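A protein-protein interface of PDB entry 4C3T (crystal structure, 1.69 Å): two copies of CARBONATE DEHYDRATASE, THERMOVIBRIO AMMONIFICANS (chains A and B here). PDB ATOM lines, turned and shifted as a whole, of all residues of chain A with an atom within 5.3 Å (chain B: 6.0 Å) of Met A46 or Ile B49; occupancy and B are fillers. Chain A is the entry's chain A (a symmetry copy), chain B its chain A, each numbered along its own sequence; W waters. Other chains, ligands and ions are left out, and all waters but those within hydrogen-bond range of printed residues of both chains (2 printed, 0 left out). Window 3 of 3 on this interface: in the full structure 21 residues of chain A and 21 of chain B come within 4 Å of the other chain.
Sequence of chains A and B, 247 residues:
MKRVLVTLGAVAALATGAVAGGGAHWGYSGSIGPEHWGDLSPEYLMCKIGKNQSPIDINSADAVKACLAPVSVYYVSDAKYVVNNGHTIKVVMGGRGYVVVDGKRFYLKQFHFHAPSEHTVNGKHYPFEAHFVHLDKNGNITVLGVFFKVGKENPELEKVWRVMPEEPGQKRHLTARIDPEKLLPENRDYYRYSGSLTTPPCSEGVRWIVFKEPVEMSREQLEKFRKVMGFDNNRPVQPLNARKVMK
Leu A45 touches its own counterpart, Leu B45. Met A46 touches Ile B49, and with the chains exchanged Ile A49 touches Met B46. Ile A49 touches its own counterpart, Ile B49. Glu A204 touches its own counterpart, Glu B204. 7 positions are printed for both chains. Of the 6 pairs that touch across the chains among the printed residues, 5 have their exchanged pair printed and touching as well.
Printed residues of chain B within 4 Å of Leu A45: Leu B45. Of the printed residues of chain B, Met A46 touches Ile B49. Printed residues of chain B within 4 Å of Ile A49: Met B46 (3.9 Å) and Ile B49 (3.1 Å). Cys A202 touches none of the printed residues of chain B. Ser A203 touches none of the printed residues of chain B. Printed residues of chain B within 4 Å of Glu A204: Lys B51 and Glu B204. Of the printed residues of chain A, Met B46 touches Ile A49. Of the printed residues of chain A, Ile B49 touches Met A46 (3.9 Å) and Ile A49 (3.1 Å). Of the printed residues of chain A, Glu B204 touches Glu A204. The nearest printed residue of chain B that does not touch Met A46 is Met B46 (5.4 Å). The nearest printed residue of chain A that does not touch Leu B45 is Ile A49 (4.5 Å).
Water W1 lies within hydrogen-bond range of the side-chain carboxylate (OE1) of Glu A204 (2.5 Å), the side-chain carboxylate (OE1) of Glu B204 (2.7 Å) and the backbone NH (N) of Lys B51 (2.8 Å). Water W2 bridges the side-chain carboxylate of Glu B204 (2.5 Å) and the side-chain carboxylate of Glu A204 (2.7 Å).
CD2 of Leu A45 touches CD2 of Leu B45 (3.5 Å). Met A46 touches Ile B49. CD1 of Ile A49 touches CE of Met B46, 3.9 Å away. Ile A49 touches Ile B49 (CD1 to CD1, 3.1 Å). Glu A204 touches Lys B51 (C to CG, 3.9 Å). Glu A204 touches Glu B204.
Hydrophobic or aromatic side chains of chain A within 4 Å of the printed part of chain B: Leu A45, Met A46 and Ile A49. Hydrophobic or aromatic side chains of chain B within 4 Å of the printed part of chain A: Leu B45, Met B46 and Ile B49. Among the printed residues, no Asp or Glu carboxylate lies within 4 Å of a Lys or Arg side-chain nitrogen of the other chain.
OE2 of Glu A204 sits at hydrogen-bond distance from NE2 of Gln A53, at 3.0 Å. OE2 of Glu B204 sits at hydrogen-bond distance from N of Lys B51 (3.4 Å).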
ATOM      1  N   GLU A  43       9.800 -20.666  -0.846  1.00  0.00           N
ATOM      2  CA  GLU A  43      11.233 -20.452  -0.653  1.00  0.00           C
ATOM      3  C   GLU A  43      11.838 -21.478   0.314  1.00  0.00           C
ATOM      4  O   GLU A  43      13.052 -21.683   0.317  1.00  0.00           O
ATOM      5  CB  GLU A  43      11.498 -19.046  -0.111  1.00  0.00           C
ATOM      6  CG  GLU A  43      10.841 -17.916  -0.892  1.00  0.00           C
ATOM      7  CD  GLU A  43      10.572 -16.699  -0.026  1.00  0.00           C
ATOM      8  OE1 GLU A  43      11.543 -16.082   0.460  1.00  0.00           O
ATOM      9  OE2 GLU A  43       9.387 -16.360   0.173  1.00  0.00           O
ATOM     10  N   TYR A  44      10.999 -22.129   1.117  1.00  0.00           N
ATOM     11  CA  TYR A  44      11.498 -23.009   2.199  1.00  0.00           C
ATOM     12  C   TYR A  44      11.486 -24.497   1.892  1.00  0.00           C
ATOM     13  O   TYR A  44      11.608 -25.330   2.785  1.00  0.00           O
ATOM     14  CB  TYR A  44      10.730 -22.768   3.521  1.00  0.00           C
ATOM     15  CG  TYR A  44      10.707 -21.357   4.053  1.00  0.00           C
ATOM     16  CD1 TYR A  44      11.589 -20.380   3.587  1.00  0.00           C
ATOM     17  CD2 TYR A  44       9.810 -21.005   5.080  1.00  0.00           C
ATOM     18  CE1 TYR A  44      11.557 -19.084   4.083  1.00  0.00           C
ATOM     19  CE2 TYR A  44       9.782 -19.712   5.588  1.00  0.00           C
ATOM     20  CZ  TYR A  44      10.657 -18.760   5.096  1.00  0.00           C
ATOM     21  OH  TYR A  44      10.658 -17.471   5.582  1.00  0.00           O
ATOM     22  N   LEU A  45      11.342 -24.850   0.621  1.00  0.00           N
ATOM     23  CA  LEU A  45      11.165 -26.249   0.257  1.00  0.00           C
ATOM     24  C   LEU A  45      12.284 -27.197   0.718  1.00  0.00           C
ATOM     25  O   LEU A  45      12.029 -28.364   1.025  1.00  0.00           O
ATOM     26  CB  LEU A  45      10.944 -26.344  -1.265  1.00  0.00           C
ATOM     27  CG  LEU A  45      10.752 -27.704  -1.931  1.00  0.00           C
ATOM     28  CD1 LEU A  45       9.463 -28.393  -1.515  1.00  0.00           C
ATOM     29  CD2 LEU A  45      10.794 -27.512  -3.437  1.00  0.00           C
ATOM     30  N   MET A  46      13.525 -26.704   0.764  1.00  0.00           N
ATOM     31  CA  MET A  46      14.671 -27.523   1.110  1.00  0.00           C
ATOM     32  C   MET A  46      14.521 -28.071   2.526  1.00  0.00           C
ATOM     33  O   MET A  46      15.005 -29.157   2.835  1.00  0.00           O
ATOM     34  CB  MET A  46      15.948 -26.684   0.989  1.00  0.00           C
ATOM     35  CG  MET A  46      17.247 -27.465   0.939  1.00  0.00           C
ATOM     36  SD  MET A  46      17.329 -28.690  -0.374  1.00  0.00           S
ATOM     37  CE  MET A  46      17.075 -27.675  -1.830  1.00  0.00           C
ATOM     38  N   CYS A  47      13.838 -27.299   3.382  1.00  0.00           N
ATOM     39  CA  CYS A  47      13.645 -27.704   4.775  1.00  0.00           C
ATOM     40  C   CYS A  47      13.043 -29.102   4.825  1.00  0.00           C
ATOM     41  O   CYS A  47      13.384 -29.897   5.707  1.00  0.00           O
ATOM     42  CB  CYS A  47      12.756 -26.703   5.542  1.00  0.00           C
ATOM     43  SG  CYS A  47      13.301 -24.973   5.601  1.00  0.00           S
ATOM     44  N   LYS A  48      12.152 -29.409   3.875  1.00  0.00           N
ATOM     45  CA  LYS A  48      11.524 -30.735   3.822  1.00  0.00           C
ATOM     46  C   LYS A  48      12.024 -31.749   2.768  1.00  0.00           C
ATOM     47  O   LYS A  48      11.886 -32.963   2.981  1.00  0.00           O
ATOM     48  CB  LYS A  48       9.998 -30.622   3.765  1.00  0.00           C
ATOM     49  CG  LYS A  48       9.427 -30.069   2.469  1.00  0.00           C
ATOM     50  CD  LYS A  48       7.912 -30.219   2.455  1.00  0.00           C
ATOM     51  CE  LYS A  48       7.282 -29.411   1.336  1.00  0.00           C
ATOM     52  NZ  LYS A  48       5.799 -29.539   1.354  1.00  0.00           N
ATOM     53  N   ILE A  49      12.577 -31.281   1.647  1.00  0.00           N
ATOM     54  CA  ILE A  49      13.045 -32.194   0.588  1.00  0.00           C
ATOM     55  C   ILE A  49      14.536 -32.509   0.699  1.00  0.00           C
ATOM     56  O   ILE A  49      15.003 -33.514   0.153  1.00  0.00           O
ATOM     57  CB  ILE A  49      12.730 -31.703  -0.855  1.00  0.00           C
ATOM     58  CG1 ILE A  49      13.433 -30.377  -1.182  1.00  0.00           C
ATOM     59  CG2 ILE A  49      11.227 -31.621  -1.094  1.00  0.00           C
ATOM     60  CD1 ILE A  49      13.461 -30.059  -2.667  1.00  0.00           C
ATOM     61  N   GLY A  50      15.272 -31.657   1.415  1.00  0.00           N
ATOM     62  CA  GLY A  50      16.727 -31.807   1.570  1.00  0.00           C
ATOM     63  C   GLY A  50      17.157 -33.089   2.258  1.00  0.00           C
ATOM     64  O   GLY A  50      16.540 -33.509   3.249  1.00  0.00           O
ATOM     65  N   GLN A  53      20.773 -31.923   5.412  1.00  0.00           N
ATOM     66  CA  GLN A  53      20.334 -30.858   6.300  1.00  0.00           C
ATOM     67  C   GLN A  53      21.143 -30.778   7.622  1.00  0.00           C
ATOM     68  O   GLN A  53      21.821 -31.724   8.005  1.00  0.00           O
ATOM     69  CB  GLN A  53      18.836 -31.043   6.606  1.00  0.00           C
ATOM     70  CG  GLN A  53      17.889 -30.735   5.440  1.00  0.00           C
ATOM     71  CD  GLN A  53      17.742 -29.250   5.190  1.00  0.00           C
ATOM     72  OE1 GLN A  53      17.095 -28.516   5.958  1.00  0.00           O
ATOM     73  NE2 GLN A  53      18.331 -28.783   4.081  1.00  0.00           N
ATOM     74  N   PRO A 201      15.714 -20.210   4.774  1.00  0.00           N
ATOM     75  CA  PRO A 201      15.272 -21.250   3.869  1.00  0.00           C
ATOM     76  C   PRO A 201      15.984 -22.620   3.911  1.00  0.00           C
ATOM     77  O   PRO A 201      15.707 -23.456   3.075  1.00  0.00           O
ATOM     78  CB  PRO A 201      15.475 -20.598   2.491  1.00  0.00           C
ATOM     79  CG  PRO A 201      16.648 -19.712   2.699  1.00  0.00           C
ATOM     80  CD  PRO A 201      16.581 -19.217   4.113  1.00  0.00           C
ATOM     81  N   CYS A 202      16.869 -22.851   4.888  1.00  0.00           N
ATOM     82  CA  CYS A 202      17.600 -24.112   5.080  1.00  0.00           C
ATOM     83  C   CYS A 202      18.319 -24.525   3.810  1.00  0.00           C
ATOM     84  O   CYS A 202      18.398 -25.686   3.467  1.00  0.00           O
ATOM     85  CB  CYS A 202      16.724 -25.250   5.587  1.00  0.00           C
ATOM     86  SG  CYS A 202      16.048 -24.831   7.207  1.00  0.00           S
ATOM     87  N   SER A 203      18.913 -23.518   3.154  1.00  0.00           N
ATOM     88  CA  SER A 203      19.691 -23.771   1.930  1.00  0.00           C
ATOM     89  C   SER A 203      20.838 -24.747   2.164  1.00  0.00           C
ATOM     90  O   SER A 203      21.516 -24.678   3.203  1.00  0.00           O
ATOM     91  CB  SER A 203      20.263 -22.460   1.381  1.00  0.00           C
ATOM     92  OG  SER A 203      19.358 -21.386   1.479  1.00  0.00           O
ATOM     93  N   GLU A 204      21.055 -25.639   1.192  1.00  0.00           N
ATOM     94  CA  GLU A 204      22.159 -26.599   1.241  1.00  0.00           C
ATOM     95  C   GLU A 204      23.414 -26.072   0.521  1.00  0.00           C
ATOM     96  O   GLU A 204      23.485 -24.882   0.193  1.00  0.00           O
ATOM     97  CB  GLU A 204      21.746 -28.001   0.781  1.00  0.00           C
ATOM     98  CG  GLU A 204      20.735 -28.659   1.735  1.00  0.00           C
ATOM     99  CD  GLU A 204      20.399 -30.097   1.403  1.00  0.00           C
ATOM    100  OE1 GLU A 204      20.854 -30.638   0.359  1.00  0.00           O
ATOM    101  OE2 GLU A 204      19.658 -30.701   2.202  1.00  0.00           O
ATOM    102  N   LEU B  45      12.885 -32.191  -9.934  1.00  0.00           N
ATOM    103  CA  LEU B  45      13.359 -30.901  -9.450  1.00  0.00           C
ATOM    104  C   LEU B  45      14.789 -30.894  -8.884  1.00  0.00           C
ATOM    105  O   LEU B  45      15.505 -29.897  -9.005  1.00  0.00           O
ATOM    106  CB  LEU B  45      12.349 -30.351  -8.423  1.00  0.00           C
ATOM    107  CG  LEU B  45      12.606 -29.016  -7.732  1.00  0.00           C
ATOM    108  CD1 LEU B  45      12.560 -27.833  -8.686  1.00  0.00           C
ATOM    109  CD2 LEU B  45      11.585 -28.846  -6.621  1.00  0.00           C
ATOM    110  N   MET B  46      15.207 -32.000  -8.261  1.00  0.00           N
ATOM    111  CA  MET B  46      16.506 -32.083  -7.622  1.00  0.00           C
ATOM    112  C   MET B  46      17.615 -31.890  -8.651  1.00  0.00           C
ATOM    113  O   MET B  46      18.686 -31.378  -8.333  1.00  0.00           O
ATOM    114  CB  MET B  46      16.644 -33.444  -6.930  1.00  0.00           C
ATOM    115  CG  MET B  46      17.757 -33.555  -5.908  1.00  0.00           C
ATOM    116  SD  MET B  46      17.684 -32.332  -4.592  1.00  0.00           S
ATOM    117  CE  MET B  46      16.066 -32.656  -3.890  1.00  0.00           C
ATOM    118  N   CYS B  47      17.339 -32.307  -9.893  1.00  0.00           N
ATOM    119  CA  CYS B  47      18.330 -32.197 -10.966  1.00  0.00           C
ATOM    120  C   CYS B  47      18.830 -30.762 -11.056  1.00  0.00           C
ATOM    121  O   CYS B  47      20.013 -30.529 -11.324  1.00  0.00           O
ATOM    122  CB  CYS B  47      17.757 -32.658 -12.322  1.00  0.00           C
ATOM    123  SG  CYS B  47      17.103 -34.348 -12.425  1.00  0.00           S
ATOM    124  N   LYS B  48      17.934 -29.795 -10.826  1.00  0.00           N
ATOM    125  CA  LYS B  48      18.316 -28.378 -10.872  1.00  0.00           C
ATOM    126  C   LYS B  48      18.509 -27.619  -9.540  1.00  0.00           C
ATOM    127  O   LYS B  48      19.257 -26.630  -9.507  1.00  0.00           O
ATOM    128  CB  LYS B  48      17.393 -27.586 -11.803  1.00  0.00           C
ATOM    129  CG  LYS B  48      15.966 -27.401 -11.312  1.00  0.00           C
ATOM    130  CD  LYS B  48      15.223 -26.419 -12.207  1.00  0.00           C
ATOM    131  CE  LYS B  48      13.730 -26.442 -11.943  1.00  0.00           C
ATOM    132  NZ  LYS B  48      13.012 -25.502 -12.849  1.00  0.00           N
ATOM    133  N   ILE B  49      17.845 -28.047  -8.462  1.00  0.00           N
ATOM    134  CA  ILE B  49      17.960 -27.349  -7.169  1.00  0.00           C
ATOM    135  C   ILE B  49      19.013 -27.973  -6.255  1.00  0.00           C
ATOM    136  O   ILE B  49      19.498 -27.319  -5.325  1.00  0.00           O
ATOM    137  CB  ILE B  49      16.615 -27.226  -6.395  1.00  0.00           C
ATOM    138  CG1 ILE B  49      16.038 -28.599  -6.017  1.00  0.00           C
ATOM    139  CG2 ILE B  49      15.609 -26.383  -7.167  1.00  0.00           C
ATOM    140  CD1 ILE B  49      14.950 -28.526  -4.959  1.00  0.00           C
ATOM    141  N   GLY B  50      19.370 -29.229  -6.531  1.00  0.00           N
ATOM    142  CA  GLY B  50      20.337 -29.973  -5.709  1.00  0.00           C
ATOM    143  C   GLY B  50      21.726 -29.362  -5.665  1.00  0.00           C
ATOM    144  O   GLY B  50      22.246 -28.907  -6.694  1.00  0.00           O
ATOM    145  N   LYS B  51      22.309 -29.323  -4.470  1.00  0.00           N
ATOM    146  CA  LYS B  51      23.680 -28.886  -4.263  1.00  0.00           C
ATOM    147  C   LYS B  51      24.651 -30.029  -3.983  1.00  0.00           C
ATOM    148  O   LYS B  51      25.824 -29.776  -3.727  1.00  0.00           O
ATOM    149  CB  LYS B  51      23.762 -27.867  -3.111  1.00  0.00           C
ATOM    150  CG  LYS B  51      22.879 -26.640  -3.280  1.00  0.00           C
ATOM    151  CD  LYS B  51      23.372 -25.788  -4.437  1.00  0.00           C
ATOM    152  CE  LYS B  51      22.445 -24.620  -4.708  1.00  0.00           C
ATOM    153  NZ  LYS B  51      22.817 -23.923  -5.970  1.00  0.00           N
ATOM    154  N   GLU B 204      18.933 -37.220  -4.153  1.00  0.00           N
ATOM    155  CA  GLU B 204      20.105 -37.101  -3.285  1.00  0.00           C
ATOM    156  C   GLU B 204      20.037 -38.066  -2.087  1.00  0.00           C
ATOM    157  O   GLU B 204      19.195 -38.971  -2.069  1.00  0.00           O
ATOM    158  CB  GLU B 204      20.394 -35.653  -2.875  1.00  0.00           C
ATOM    159  CG  GLU B 204      20.814 -34.776  -4.067  1.00  0.00           C
ATOM    160  CD  GLU B 204      21.245 -33.373  -3.697  1.00  0.00           C
ATOM    161  OE1 GLU B 204      21.150 -32.965  -2.508  1.00  0.00           O
ATOM    162  OE2 GLU B 204      21.684 -32.658  -4.618  1.00  0.00           O
HETATM  163  O   HOH W   1      21.339 -30.358  -2.063  1.00  0.00           O
HETATM  164  O   HOH W   2      19.750 -32.907  -0.455  1.00  0.00           O
